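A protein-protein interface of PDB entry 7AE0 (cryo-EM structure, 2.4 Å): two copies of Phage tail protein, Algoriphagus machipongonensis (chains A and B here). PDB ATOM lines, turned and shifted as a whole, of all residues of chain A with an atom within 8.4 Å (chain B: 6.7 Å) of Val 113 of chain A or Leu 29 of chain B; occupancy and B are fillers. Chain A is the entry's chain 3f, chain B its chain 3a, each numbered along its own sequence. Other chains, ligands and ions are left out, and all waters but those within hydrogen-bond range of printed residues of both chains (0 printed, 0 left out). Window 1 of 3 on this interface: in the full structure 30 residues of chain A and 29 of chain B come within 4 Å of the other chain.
Among the printed residues, pairs that only touch across the chains: Phe 72 of chain A with Ile 139 of chain B (3.9 Å), Tyr 75 of chain A with Glu 30 of chain B (3.5 Å), Leu 111 of chain A with Glu 30 of chain B (3.8 Å), Lys 112 of chain A with Leu 29 of chain B (3.1 Å) and Ser 115 of chain A with Ile 139 of chain B (3.9 Å).
The side-chain amino group (NZ) of Lys 54 of chain B is in salt-bridge range of the side-chain carboxylate (OE2) of Glu 30 of chain B. N of Leu 111 of chain A is in hydrogen-bond range of O of Glu 131 of chain A (2.9 Å). The side-chain amino group (NZ) of Lys 112 of chain A lies close to the side-chain amide nitrogen (NE2) of Gln 114 of chain A (3.4 Å). OE1 of Glu 131 of chain A lies within salt-bridge range of NZ of Lys 112 of chain A (3.3 Å). The backbone NH (N) of Gln 114 of chain A is in hydrogen-bond range of the backbone carbonyl oxygen (O) of Ser 129 of chain A, 2.9 Å away.
No position is printed for both chains. Of the 11 pairs that touch across the chains among the printed residues, none has its exchanged pair printed and touching as well.
Tyr 71 of chain A touches none of the printed residues of chain B. Val 113 of chain A touches just one residue of chain B: Leu 29 (3.3 Å). Printed residues of chain A within 4 Å of Leu 27 of chain B: Ser 115. Leu 29 of chain B touches just these residues of chain A: Lys 112 and Val 113. Val 138 of chain B touches none of the printed residues of chain A. Of the printed residues of chain A, Ile 139 of chain B touches Asn 69, Phe 72 and Ser 115. The nearest residue of chain B that does not touch Val 113 of chain A is Asp 28 of chain B (4.1 Å). The nearest printed residue of chain B that does not touch Ser 115 of chain A is Asp 28 of chain B (4.1 Å).
Hydrophobic or aromatic side chains of chain B within 4 Å of the printed part of chain A: Leu 29 and Ile 139. Among the printed residues, 11 pairs touch across the chains. Among the printed residues, no Asp or Glu carboxylate lies within 4 Å of a Lys or Arg side-chain nitrogen of the other chain.
O of Leu 27 of chain B lies close to OG of Ser 115 of chain A, at 3.4 Å. The side-chain carboxylate of Asp 28 of chain B lies within hydrogen-bond range of the side-chain amide nitrogen of Gln 114 of chain A. N of Leu 29 of chain B sits at hydrogen-bond distance from O of Val 113 of chain A (3.3 Å). OG1 of Thr 31 of chain B is in hydrogen-bond range of OH of Tyr 75 of chain A, 2.8 Å away. The backbone carbonyl oxygen (O) of Leu 111 of chain A lies within hydrogen-bond range of the backbone NH (N) of Thr 31 of chain B (3.0 Å). The side-chain amide nitrogen (ND2) of Asn 69 of chain A lies within hydrogen-bond range of the backbone carbonyl oxygen (O) of Ile 139 of chain B, 3.2 Å away.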
ATOM      1  N   LEU A  60      -3.976 -13.586   3.647  1.00  0.00           N
ATOM      2  CA  LEU A  60      -5.068 -14.058   4.500  1.00  0.00           C
ATOM      3  C   LEU A  60      -4.563 -14.545   5.865  1.00  0.00           C
ATOM      4  O   LEU A  60      -3.600 -15.315   5.935  1.00  0.00           O
ATOM      5  CB  LEU A  60      -5.813 -15.209   3.804  1.00  0.00           C
ATOM      6  CG  LEU A  60      -6.444 -14.970   2.407  1.00  0.00           C
ATOM      7  CD1 LEU A  60      -6.976 -16.277   1.859  1.00  0.00           C
ATOM      8  CD2 LEU A  60      -7.565 -13.973   2.492  1.00  0.00           C
ATOM      9  N   ASN A  69      -5.624 -28.724   9.045  1.00  0.00           N
ATOM     10  CA  ASN A  69      -4.304 -28.562   8.433  1.00  0.00           C
ATOM     11  C   ASN A  69      -4.383 -28.053   6.967  1.00  0.00           C
ATOM     12  O   ASN A  69      -3.458 -28.242   6.191  1.00  0.00           O
ATOM     13  CB  ASN A  69      -3.520 -29.885   8.579  1.00  0.00           C
ATOM     14  CG  ASN A  69      -2.001 -29.695   8.584  1.00  0.00           C
ATOM     15  OD1 ASN A  69      -1.501 -28.675   8.989  1.00  0.00           O
ATOM     16  ND2 ASN A  69      -1.277 -30.685   8.116  1.00  0.00           N
ATOM     17  N   GLU A  70      -5.442 -27.314   6.627  1.00  0.00           N
ATOM     18  CA  GLU A  70      -5.694 -26.906   5.233  1.00  0.00           C
ATOM     19  C   GLU A  70      -4.645 -26.001   4.560  1.00  0.00           C
ATOM     20  O   GLU A  70      -4.355 -26.218   3.377  1.00  0.00           O
ATOM     21  CB  GLU A  70      -7.089 -26.290   5.094  1.00  0.00           C
ATOM     22  CG  GLU A  70      -8.218 -27.251   5.433  1.00  0.00           C
ATOM     23  CD  GLU A  70      -9.586 -26.633   5.231  1.00  0.00           C
ATOM     24  OE1 GLU A  70      -9.656 -25.416   4.962  1.00  0.00           O
ATOM     25  OE2 GLU A  70     -10.588 -27.341   5.427  1.00  0.00           O
ATOM     26  N   TYR A  71      -4.093 -24.999   5.247  1.00  0.00           N
ATOM     27  CA  TYR A  71      -3.075 -24.177   4.620  1.00  0.00           C
ATOM     28  C   TYR A  71      -1.961 -25.069   4.100  1.00  0.00           C
ATOM     29  O   TYR A  71      -1.522 -24.934   2.969  1.00  0.00           O
ATOM     30  CB  TYR A  71      -2.464 -23.202   5.627  1.00  0.00           C
ATOM     31  CG  TYR A  71      -3.179 -21.900   5.865  1.00  0.00           C
ATOM     32  CD1 TYR A  71      -2.502 -20.811   6.400  1.00  0.00           C
ATOM     33  CD2 TYR A  71      -4.514 -21.739   5.547  1.00  0.00           C
ATOM     34  CE1 TYR A  71      -3.142 -19.620   6.633  1.00  0.00           C
ATOM     35  CE2 TYR A  71      -5.151 -20.551   5.771  1.00  0.00           C
ATOM     36  CZ  TYR A  71      -4.455 -19.492   6.300  1.00  0.00           C
ATOM     37  OH  TYR A  71      -5.087 -18.314   6.534  1.00  0.00           O
ATOM     38  N   PHE A  72      -1.576 -26.058   4.898  1.00  0.00           N
ATOM     39  CA  PHE A  72      -0.470 -26.912   4.533  1.00  0.00           C
ATOM     40  C   PHE A  72      -0.852 -27.809   3.384  1.00  0.00           C
ATOM     41  O   PHE A  72      -0.078 -27.972   2.444  1.00  0.00           O
ATOM     42  CB  PHE A  72       0.017 -27.746   5.706  1.00  0.00           C
ATOM     43  CG  PHE A  72       1.176 -28.611   5.344  1.00  0.00           C
ATOM     44  CD1 PHE A  72       2.434 -28.069   5.206  1.00  0.00           C
ATOM     45  CD2 PHE A  72       1.011 -29.956   5.106  1.00  0.00           C
ATOM     46  CE1 PHE A  72       3.496 -28.854   4.845  1.00  0.00           C
ATOM     47  CE2 PHE A  72       2.069 -30.740   4.745  1.00  0.00           C
ATOM     48  CZ  PHE A  72       3.311 -30.190   4.614  1.00  0.00           C
ATOM     49  N   GLN A  73      -2.037 -28.410   3.460  1.00  0.00           N
ATOM     50  CA  GLN A  73      -2.465 -29.339   2.433  1.00  0.00           C
ATOM     51  C   GLN A  73      -2.555 -28.694   1.053  1.00  0.00           C
ATOM     52  O   GLN A  73      -2.180 -29.322   0.066  1.00  0.00           O
ATOM     53  CB  GLN A  73      -3.805 -29.934   2.822  1.00  0.00           C
ATOM     54  CG  GLN A  73      -3.739 -30.891   4.000  1.00  0.00           C
ATOM     55  CD  GLN A  73      -5.111 -31.276   4.450  1.00  0.00           C
ATOM     56  OE1 GLN A  73      -6.084 -30.678   3.997  1.00  0.00           O
ATOM     57  NE2 GLN A  73      -5.212 -32.259   5.331  1.00  0.00           N
ATOM     58  N   TRP A  74      -3.042 -27.449   0.956  1.00  0.00           N
ATOM     59  CA  TRP A  74      -3.082 -26.781  -0.344  1.00  0.00           C
ATOM     60  C   TRP A  74      -1.654 -26.518  -0.850  1.00  0.00           C
ATOM     61  O   TRP A  74      -1.336 -26.779  -2.018  1.00  0.00           O
ATOM     62  CB  TRP A  74      -3.910 -25.483  -0.278  1.00  0.00           C
ATOM     63  CG  TRP A  74      -4.178 -24.791  -1.638  1.00  0.00           C
ATOM     64  CD1 TRP A  74      -3.974 -25.302  -2.883  1.00  0.00           C
ATOM     65  CD2 TRP A  74      -4.717 -23.475  -1.851  1.00  0.00           C
ATOM     66  NE1 TRP A  74      -4.331 -24.402  -3.830  1.00  0.00           N
ATOM     67  CE2 TRP A  74      -4.796 -23.279  -3.228  1.00  0.00           C
ATOM     68  CE3 TRP A  74      -5.134 -22.452  -1.008  1.00  0.00           C
ATOM     69  CZ2 TRP A  74      -5.270 -22.115  -3.784  1.00  0.00           C
ATOM     70  CZ3 TRP A  74      -5.611 -21.293  -1.566  1.00  0.00           C
ATOM     71  CH2 TRP A  74      -5.673 -21.131  -2.930  1.00  0.00           C
ATOM     72  N   TYR A  75      -0.790 -25.994   0.026  1.00  0.00           N
ATOM     73  CA  TYR A  75       0.599 -25.694  -0.321  1.00  0.00           C
ATOM     74  C   TYR A  75       1.313 -26.935  -0.833  1.00  0.00           C
ATOM     75  O   TYR A  75       2.050 -26.901  -1.823  1.00  0.00           O
ATOM     76  CB  TYR A  75       1.340 -25.129   0.888  1.00  0.00           C
ATOM     77  CG  TYR A  75       2.717 -24.644   0.566  1.00  0.00           C
ATOM     78  CD1 TYR A  75       2.882 -23.382   0.030  1.00  0.00           C
ATOM     79  CD2 TYR A  75       3.826 -25.437   0.777  1.00  0.00           C
ATOM     80  CE1 TYR A  75       4.110 -22.910  -0.288  1.00  0.00           C
ATOM     81  CE2 TYR A  75       5.071 -24.970   0.455  1.00  0.00           C
ATOM     82  CZ  TYR A  75       5.208 -23.705  -0.078  1.00  0.00           C
ATOM     83  OH  TYR A  75       6.444 -23.230  -0.401  1.00  0.00           O
ATOM     84  N   ASN A  76       1.046 -28.057  -0.198  1.00  0.00           N
ATOM     85  CA  ASN A  76       1.671 -29.326  -0.510  1.00  0.00           C
ATOM     86  C   ASN A  76       1.166 -29.947  -1.830  1.00  0.00           C
ATOM     87  O   ASN A  76       1.611 -31.040  -2.186  1.00  0.00           O
ATOM     88  CB  ASN A  76       1.454 -30.257   0.680  1.00  0.00           C
ATOM     89  CG  ASN A  76       2.414 -31.406   0.757  1.00  0.00           C
ATOM     90  OD1 ASN A  76       3.630 -31.244   0.651  1.00  0.00           O
ATOM     91  ND2 ASN A  76       1.878 -32.582   0.966  1.00  0.00           N
ATOM     92  N   ILE A  78       1.930 -28.536  -4.648  1.00  0.00           N
ATOM     93  CA  ILE A  78       2.928 -28.068  -5.626  1.00  0.00           C
ATOM     94  C   ILE A  78       3.835 -29.222  -6.055  1.00  0.00           C
ATOM     95  O   ILE A  78       4.376 -29.924  -5.224  1.00  0.00           O
ATOM     96  CB  ILE A  78       3.772 -26.902  -5.056  1.00  0.00           C
ATOM     97  CG1 ILE A  78       3.012 -25.577  -5.096  1.00  0.00           C
ATOM     98  CG2 ILE A  78       5.111 -26.751  -5.779  1.00  0.00           C
ATOM     99  CD1 ILE A  78       3.461 -24.544  -4.082  1.00  0.00           C
ATOM    100  N   PRO A 110      -0.815 -20.672  -3.579  1.00  0.00           N
ATOM    101  CA  PRO A 110       0.036 -20.108  -2.495  1.00  0.00           C
ATOM    102  C   PRO A 110       1.571 -20.018  -2.612  1.00  0.00           C
ATOM    103  O   PRO A 110       2.246 -21.002  -2.791  1.00  0.00           O
ATOM    104  CB  PRO A 110      -0.299 -21.009  -1.305  1.00  0.00           C
ATOM    105  CG  PRO A 110      -1.024 -22.202  -1.849  1.00  0.00           C
ATOM    106  CD  PRO A 110      -1.255 -22.047  -3.298  1.00  0.00           C
ATOM    107  N   LEU A 111       2.114 -18.811  -2.559  1.00  0.00           N
ATOM    108  CA  LEU A 111       3.565 -18.588  -2.531  1.00  0.00           C
ATOM    109  C   LEU A 111       4.182 -18.950  -1.208  1.00  0.00           C
ATOM    110  O   LEU A 111       5.302 -19.422  -1.168  1.00  0.00           O
ATOM    111  CB  LEU A 111       3.907 -17.128  -2.780  1.00  0.00           C
ATOM    112  CG  LEU A 111       3.601 -16.675  -4.172  1.00  0.00           C
ATOM    113  CD1 LEU A 111       3.308 -15.186  -4.140  1.00  0.00           C
ATOM    114  CD2 LEU A 111       4.717 -17.055  -5.128  1.00  0.00           C
ATOM    115  N   LYS A 112       3.499 -18.631  -0.120  1.00  0.00           N
ATOM    116  CA  LYS A 112       4.051 -18.970   1.169  1.00  0.00           C
ATOM    117  C   LYS A 112       3.070 -19.134   2.315  1.00  0.00           C
ATOM    118  O   LYS A 112       2.031 -18.506   2.390  1.00  0.00           O
ATOM    119  CB  LYS A 112       5.183 -18.033   1.562  1.00  0.00           C
ATOM    120  CG  LYS A 112       4.878 -16.613   1.848  1.00  0.00           C
ATOM    121  CD  LYS A 112       6.153 -16.063   2.447  1.00  0.00           C
ATOM    122  CE  LYS A 112       6.118 -14.574   2.651  1.00  0.00           C
ATOM    123  NZ  LYS A 112       5.164 -14.169   3.714  1.00  0.00           N
ATOM    124  N   VAL A 113       3.452 -20.020   3.213  1.00  0.00           N
ATOM    125  CA  VAL A 113       2.680 -20.334   4.407  1.00  0.00           C
ATOM    126  C   VAL A 113       3.552 -20.026   5.620  1.00  0.00           C
ATOM    127  O   VAL A 113       4.668 -20.538   5.728  1.00  0.00           O
ATOM    128  CB  VAL A 113       2.200 -21.798   4.408  1.00  0.00           C
ATOM    129  CG1 VAL A 113       1.429 -22.110   5.687  1.00  0.00           C
ATOM    130  CG2 VAL A 113       1.301 -22.036   3.218  1.00  0.00           C
ATOM    131  N   GLN A 114       3.079 -19.134   6.502  1.00  0.00           N
ATOM    132  CA  GLN A 114       3.832 -18.745   7.713  1.00  0.00           C
ATOM    133  C   GLN A 114       3.153 -19.202   9.006  1.00  0.00           C
ATOM    134  O   GLN A 114       1.981 -18.915   9.243  1.00  0.00           O
ATOM    135  CB  GLN A 114       4.134 -17.241   7.753  1.00  0.00           C
ATOM    136  CG  GLN A 114       5.141 -16.853   6.682  1.00  0.00           C
ATOM    137  CD  GLN A 114       5.687 -15.455   6.809  1.00  0.00           C
ATOM    138  OE1 GLN A 114       5.015 -14.551   7.277  1.00  0.00           O
ATOM    139  NE2 GLN A 114       6.922 -15.269   6.372  1.00  0.00           N
ATOM    140  N   SER A 115       3.913 -19.922   9.817  1.00  0.00           N
ATOM    141  CA  SER A 115       3.483 -20.393  11.127  1.00  0.00           C
ATOM    142  C   SER A 115       3.748 -19.364  12.219  1.00  0.00           C
ATOM    143  O   SER A 115       4.470 -18.382  12.032  1.00  0.00           O
ATOM    144  CB  SER A 115       4.175 -21.696  11.492  1.00  0.00           C
ATOM    145  OG  SER A 115       3.801 -22.729  10.627  1.00  0.00           O
ATOM    146  N   THR A 116       3.133 -19.634  13.366  1.00  0.00           N
ATOM    147  CA  THR A 116       3.209 -18.881  14.622  1.00  0.00           C
ATOM    148  C   THR A 116       4.550 -18.983  15.386  1.00  0.00           C
ATOM    149  O   THR A 116       5.275 -19.970  15.283  1.00  0.00           O
ATOM    150  CB  THR A 116       2.074 -19.408  15.536  1.00  0.00           C
ATOM    151  OG1 THR A 116       1.775 -18.474  16.566  1.00  0.00           O
ATOM    152  CG2 THR A 116       2.426 -20.762  16.186  1.00  0.00           C
ATOM    153  N   GLU A 128      -1.956 -18.142  12.156  1.00  0.00           N
ATOM    154  CA  GLU A 128      -1.238 -18.553  10.954  1.00  0.00           C
ATOM    155  C   GLU A 128      -1.656 -17.702   9.756  1.00  0.00           C
ATOM    156  O   GLU A 128      -2.791 -17.214   9.695  1.00  0.00           O
ATOM    157  CB  GLU A 128      -1.493 -20.030  10.651  1.00  0.00           C
ATOM    158  CG  GLU A 128      -2.960 -20.398  10.451  1.00  0.00           C
ATOM    159  CD  GLU A 128      -3.149 -21.823  10.042  1.00  0.00           C
ATOM    160  OE1 GLU A 128      -2.169 -22.523   9.871  1.00  0.00           O
ATOM    161  OE2 GLU A 128      -4.277 -22.235   9.884  1.00  0.00           O
ATOM    162  N   SER A 129      -0.760 -17.587   8.763  1.00  0.00           N
ATOM    163  CA  SER A 129      -1.072 -16.801   7.570  1.00  0.00           C
ATOM    164  C   SER A 129      -0.554 -17.367   6.245  1.00  0.00           C
ATOM    165  O   SER A 129       0.413 -18.127   6.177  1.00  0.00           O
ATOM    166  CB  SER A 129      -0.532 -15.402   7.725  1.00  0.00           C
ATOM    167  OG  SER A 129       0.858 -15.403   7.747  1.00  0.00           O
ATOM    168  N   MET A 130      -1.216 -16.944   5.169  1.00  0.00           N
ATOM    169  CA  MET A 130      -0.898 -17.362   3.807  1.00  0.00           C
ATOM    170  C   MET A 130      -0.853 -16.208   2.797  1.00  0.00           C
ATOM    171  O   MET A 130      -1.680 -15.294   2.831  1.00  0.00           O
ATOM    172  CB  MET A 130      -1.933 -18.406   3.379  1.00  0.00           C
ATOM    173  CG  MET A 130      -1.841 -18.911   1.956  1.00  0.00           C
ATOM    174  SD  MET A 130      -3.104 -20.141   1.576  1.00  0.00           S
ATOM    175  CE  MET A 130      -2.361 -21.639   2.121  1.00  0.00           C
ATOM    176  N   GLU A 131       0.097 -16.282   1.858  1.00  0.00           N
ATOM    177  CA  GLU A 131       0.214 -15.305   0.771  1.00  0.00           C
ATOM    178  C   GLU A 131      -0.059 -15.945  -0.597  1.00  0.00           C
ATOM    179  O   GLU A 131       0.574 -16.943  -0.972  1.00  0.00           O
ATOM    180  CB  GLU A 131       1.589 -14.642   0.801  1.00  0.00           C
ATOM    181  CG  GLU A 131       1.823 -13.566  -0.243  1.00  0.00           C
ATOM    182  CD  GLU A 131       3.173 -12.914  -0.074  1.00  0.00           C
ATOM    183  OE1 GLU A 131       3.795 -13.174   0.934  1.00  0.00           O
ATOM    184  OE2 GLU A 131       3.610 -12.161  -0.939  1.00  0.00           O
ATOM    185  N   LEU A 132      -1.004 -15.357  -1.339  1.00  0.00           N
ATOM    186  CA  LEU A 132      -1.447 -15.873  -2.636  1.00  0.00           C
ATOM    187  C   LEU A 132      -1.101 -15.044  -3.881  1.00  0.00           C
ATOM    188  O   LEU A 132      -1.356 -13.839  -3.956  1.00  0.00           O
ATOM    189  CB  LEU A 132      -2.974 -16.019  -2.642  1.00  0.00           C
ATOM    190  CG  LEU A 132      -3.647 -16.937  -1.604  1.00  0.00           C
ATOM    191  CD1 LEU A 132      -5.136 -16.793  -1.709  1.00  0.00           C
ATOM    192  CD2 LEU A 132      -3.272 -18.363  -1.846  1.00  0.00           C
ATOM    193  N   GLY B  26      10.680 -18.647  13.349  1.00  0.00           N
ATOM    194  CA  GLY B  26      11.208 -18.925  12.002  1.00  0.00           C
ATOM    195  C   GLY B  26      10.647 -20.152  11.268  1.00  0.00           C
ATOM    196  O   GLY B  26      11.201 -20.566  10.248  1.00  0.00           O
ATOM    197  N   LEU B  27       9.544 -20.722  11.725  1.00  0.00           N
ATOM    198  CA  LEU B  27       8.963 -21.912  11.090  1.00  0.00           C
ATOM    199  C   LEU B  27       8.168 -21.587   9.808  1.00  0.00           C
ATOM    200  O   LEU B  27       6.952 -21.776   9.744  1.00  0.00           O
ATOM    201  CB  LEU B  27       8.078 -22.605  12.128  1.00  0.00           C
ATOM    202  CG  LEU B  27       8.782 -23.072  13.449  1.00  0.00           C
ATOM    203  CD1 LEU B  27       7.759 -23.561  14.457  1.00  0.00           C
ATOM    204  CD2 LEU B  27       9.766 -24.193  13.151  1.00  0.00           C
ATOM    205  N   ASP B  28       8.893 -21.123   8.774  1.00  0.00           N
ATOM    206  CA  ASP B  28       8.353 -20.669   7.483  1.00  0.00           C
ATOM    207  C   ASP B  28       8.660 -21.565   6.271  1.00  0.00           C
ATOM    208  O   ASP B  28       9.649 -22.298   6.244  1.00  0.00           O
ATOM    209  CB  ASP B  28       8.896 -19.275   7.124  1.00  0.00           C
ATOM    210  CG  ASP B  28       8.474 -18.190   8.099  1.00  0.00           C
ATOM    211  OD1 ASP B  28       7.708 -18.494   9.035  1.00  0.00           O
ATOM    212  OD2 ASP B  28       8.870 -17.022   7.896  1.00  0.00           O
ATOM    213  N   LEU B  29       7.800 -21.471   5.246  1.00  0.00           N
ATOM    214  CA  LEU B  29       7.940 -22.165   3.957  1.00  0.00           C
ATOM    215  C   LEU B  29       7.807 -21.154   2.815  1.00  0.00           C
ATOM    216  O   LEU B  29       6.880 -20.346   2.844  1.00  0.00           O
ATOM    217  CB  LEU B  29       6.828 -23.220   3.813  1.00  0.00           C
ATOM    218  CG  LEU B  29       6.744 -24.335   4.886  1.00  0.00           C
ATOM    219  CD1 LEU B  29       5.458 -25.098   4.735  1.00  0.00           C
ATOM    220  CD2 LEU B  29       7.882 -25.277   4.742  1.00  0.00           C
ATOM    221  N   GLU B  30       8.668 -21.201   1.780  1.00  0.00           N
ATOM    222  CA  GLU B  30       8.552 -20.221   0.684  1.00  0.00           C
ATOM    223  C   GLU B  30       8.894 -20.763  -0.719  1.00  0.00           C
ATOM    224  O   GLU B  30       9.841 -21.528  -0.897  1.00  0.00           O
ATOM    225  CB  GLU B  30       9.423 -19.013   1.015  1.00  0.00           C
ATOM    226  CG  GLU B  30       9.411 -17.896   0.012  1.00  0.00           C
ATOM    227  CD  GLU B  30      10.189 -16.717   0.488  1.00  0.00           C
ATOM    228  OE1 GLU B  30      10.746 -16.780   1.561  1.00  0.00           O
ATOM    229  OE2 GLU B  30      10.428 -15.826  -0.306  1.00  0.00           O
ATOM    230  N   THR B  31       8.117 -20.353  -1.720  1.00  0.00           N
ATOM    231  CA  THR B  31       8.325 -20.738  -3.122  1.00  0.00           C
ATOM    232  C   THR B  31       8.517 -19.531  -4.054  1.00  0.00           C
ATOM    233  O   THR B  31       7.829 -18.526  -3.916  1.00  0.00           O
ATOM    234  CB  THR B  31       7.146 -21.590  -3.661  1.00  0.00           C
ATOM    235  OG1 THR B  31       7.202 -22.898  -3.102  1.00  0.00           O
ATOM    236  CG2 THR B  31       7.209 -21.747  -5.161  1.00  0.00           C
ATOM    237  N   LYS B  54      12.525 -22.553  -0.809  1.00  0.00           N
ATOM    238  CA  LYS B  54      13.384 -22.079   0.281  1.00  0.00           C
ATOM    239  C   LYS B  54      12.842 -22.376   1.679  1.00  0.00           C
ATOM    240  O   LYS B  54      11.635 -22.532   1.895  1.00  0.00           O
ATOM    241  CB  LYS B  54      13.562 -20.575   0.210  1.00  0.00           C
ATOM    242  CG  LYS B  54      14.312 -20.068  -0.965  1.00  0.00           C
ATOM    243  CD  LYS B  54      14.275 -18.549  -1.009  1.00  0.00           C
ATOM    244  CE  LYS B  54      12.941 -18.064  -1.560  1.00  0.00           C
ATOM    245  NZ  LYS B  54      12.897 -16.579  -1.779  1.00  0.00           N
ATOM    246  N   PHE B  55      13.758 -22.379   2.649  1.00  0.00           N
ATOM    247  CA  PHE B  55      13.414 -22.485   4.063  1.00  0.00           C
ATOM    248  C   PHE B  55      14.123 -21.397   4.861  1.00  0.00           C
ATOM    249  O   PHE B  55      15.232 -21.001   4.514  1.00  0.00           O
ATOM    250  CB  PHE B  55      13.805 -23.845   4.615  1.00  0.00           C
ATOM    251  CG  PHE B  55      13.129 -24.960   3.936  1.00  0.00           C
ATOM    252  CD1 PHE B  55      13.772 -25.662   2.945  1.00  0.00           C
ATOM    253  CD2 PHE B  55      11.831 -25.283   4.244  1.00  0.00           C
ATOM    254  CE1 PHE B  55      13.140 -26.662   2.283  1.00  0.00           C
ATOM    255  CE2 PHE B  55      11.195 -26.287   3.579  1.00  0.00           C
ATOM    256  CZ  PHE B  55      11.847 -26.974   2.596  1.00  0.00           C
ATOM    257  N   SER B  56      13.502 -20.935   5.947  1.00  0.00           N
ATOM    258  CA  SER B  56      14.116 -19.953   6.845  1.00  0.00           C
ATOM    259  C   SER B  56      14.907 -20.622   7.968  1.00  0.00           C
ATOM    260  O   SER B  56      14.646 -21.771   8.326  1.00  0.00           O
ATOM    261  CB  SER B  56      13.060 -19.059   7.477  1.00  0.00           C
ATOM    262  OG  SER B  56      12.420 -18.264   6.519  1.00  0.00           O
ATOM    263  N   GLY B 136      14.588 -28.832   5.597  1.00  0.00           N
ATOM    264  CA  GLY B 136      13.204 -29.168   5.310  1.00  0.00           C
ATOM    265  C   GLY B 136      12.291 -29.255   6.514  1.00  0.00           C
ATOM    266  O   GLY B 136      12.675 -29.707   7.593  1.00  0.00           O
ATOM    267  N   LEU B 137      11.036 -28.863   6.285  1.00  0.00           N
ATOM    268  CA  LEU B 137       9.991 -28.790   7.298  1.00  0.00           C
ATOM    269  C   LEU B 137       8.662 -29.407   6.859  1.00  0.00           C
ATOM    270  O   LEU B 137       8.120 -29.069   5.805  1.00  0.00           O
ATOM    271  CB  LEU B 137       9.778 -27.317   7.699  1.00  0.00           C
ATOM    272  CG  LEU B 137       8.572 -26.963   8.605  1.00  0.00           C
ATOM    273  CD1 LEU B 137       8.710 -27.603   9.962  1.00  0.00           C
ATOM    274  CD2 LEU B 137       8.471 -25.434   8.757  1.00  0.00           C
ATOM    275  N   VAL B 138       8.124 -30.278   7.712  1.00  0.00           N
ATOM    276  CA  VAL B 138       6.818 -30.914   7.530  1.00  0.00           C
ATOM    277  C   VAL B 138       5.895 -30.572   8.706  1.00  0.00           C
ATOM    278  O   VAL B 138       6.306 -30.636   9.869  1.00  0.00           O
ATOM    279  CB  VAL B 138       6.959 -32.442   7.364  1.00  0.00           C
ATOM    280  CG1 VAL B 138       5.600 -33.110   7.259  1.00  0.00           C
ATOM    281  CG2 VAL B 138       7.760 -32.737   6.120  1.00  0.00           C
ATOM    282  N   ILE B 139       4.655 -30.183   8.416  1.00  0.00           N
ATOM    283  CA  ILE B 139       3.718 -29.803   9.478  1.00  0.00           C
ATOM    284  C   ILE B 139       2.600 -30.827   9.654  1.00  0.00           C
ATOM    285  O   ILE B 139       1.854 -31.114   8.717  1.00  0.00           O
ATOM    286  CB  ILE B 139       3.114 -28.421   9.214  1.00  0.00           C
ATOM    287  CG1 ILE B 139       4.250 -27.398   9.096  1.00  0.00           C
ATOM    288  CG2 ILE B 139       2.164 -28.047  10.386  1.00  0.00           C
ATOM    289  CD1 ILE B 139       3.857 -26.038   8.600  1.00  0.00           C
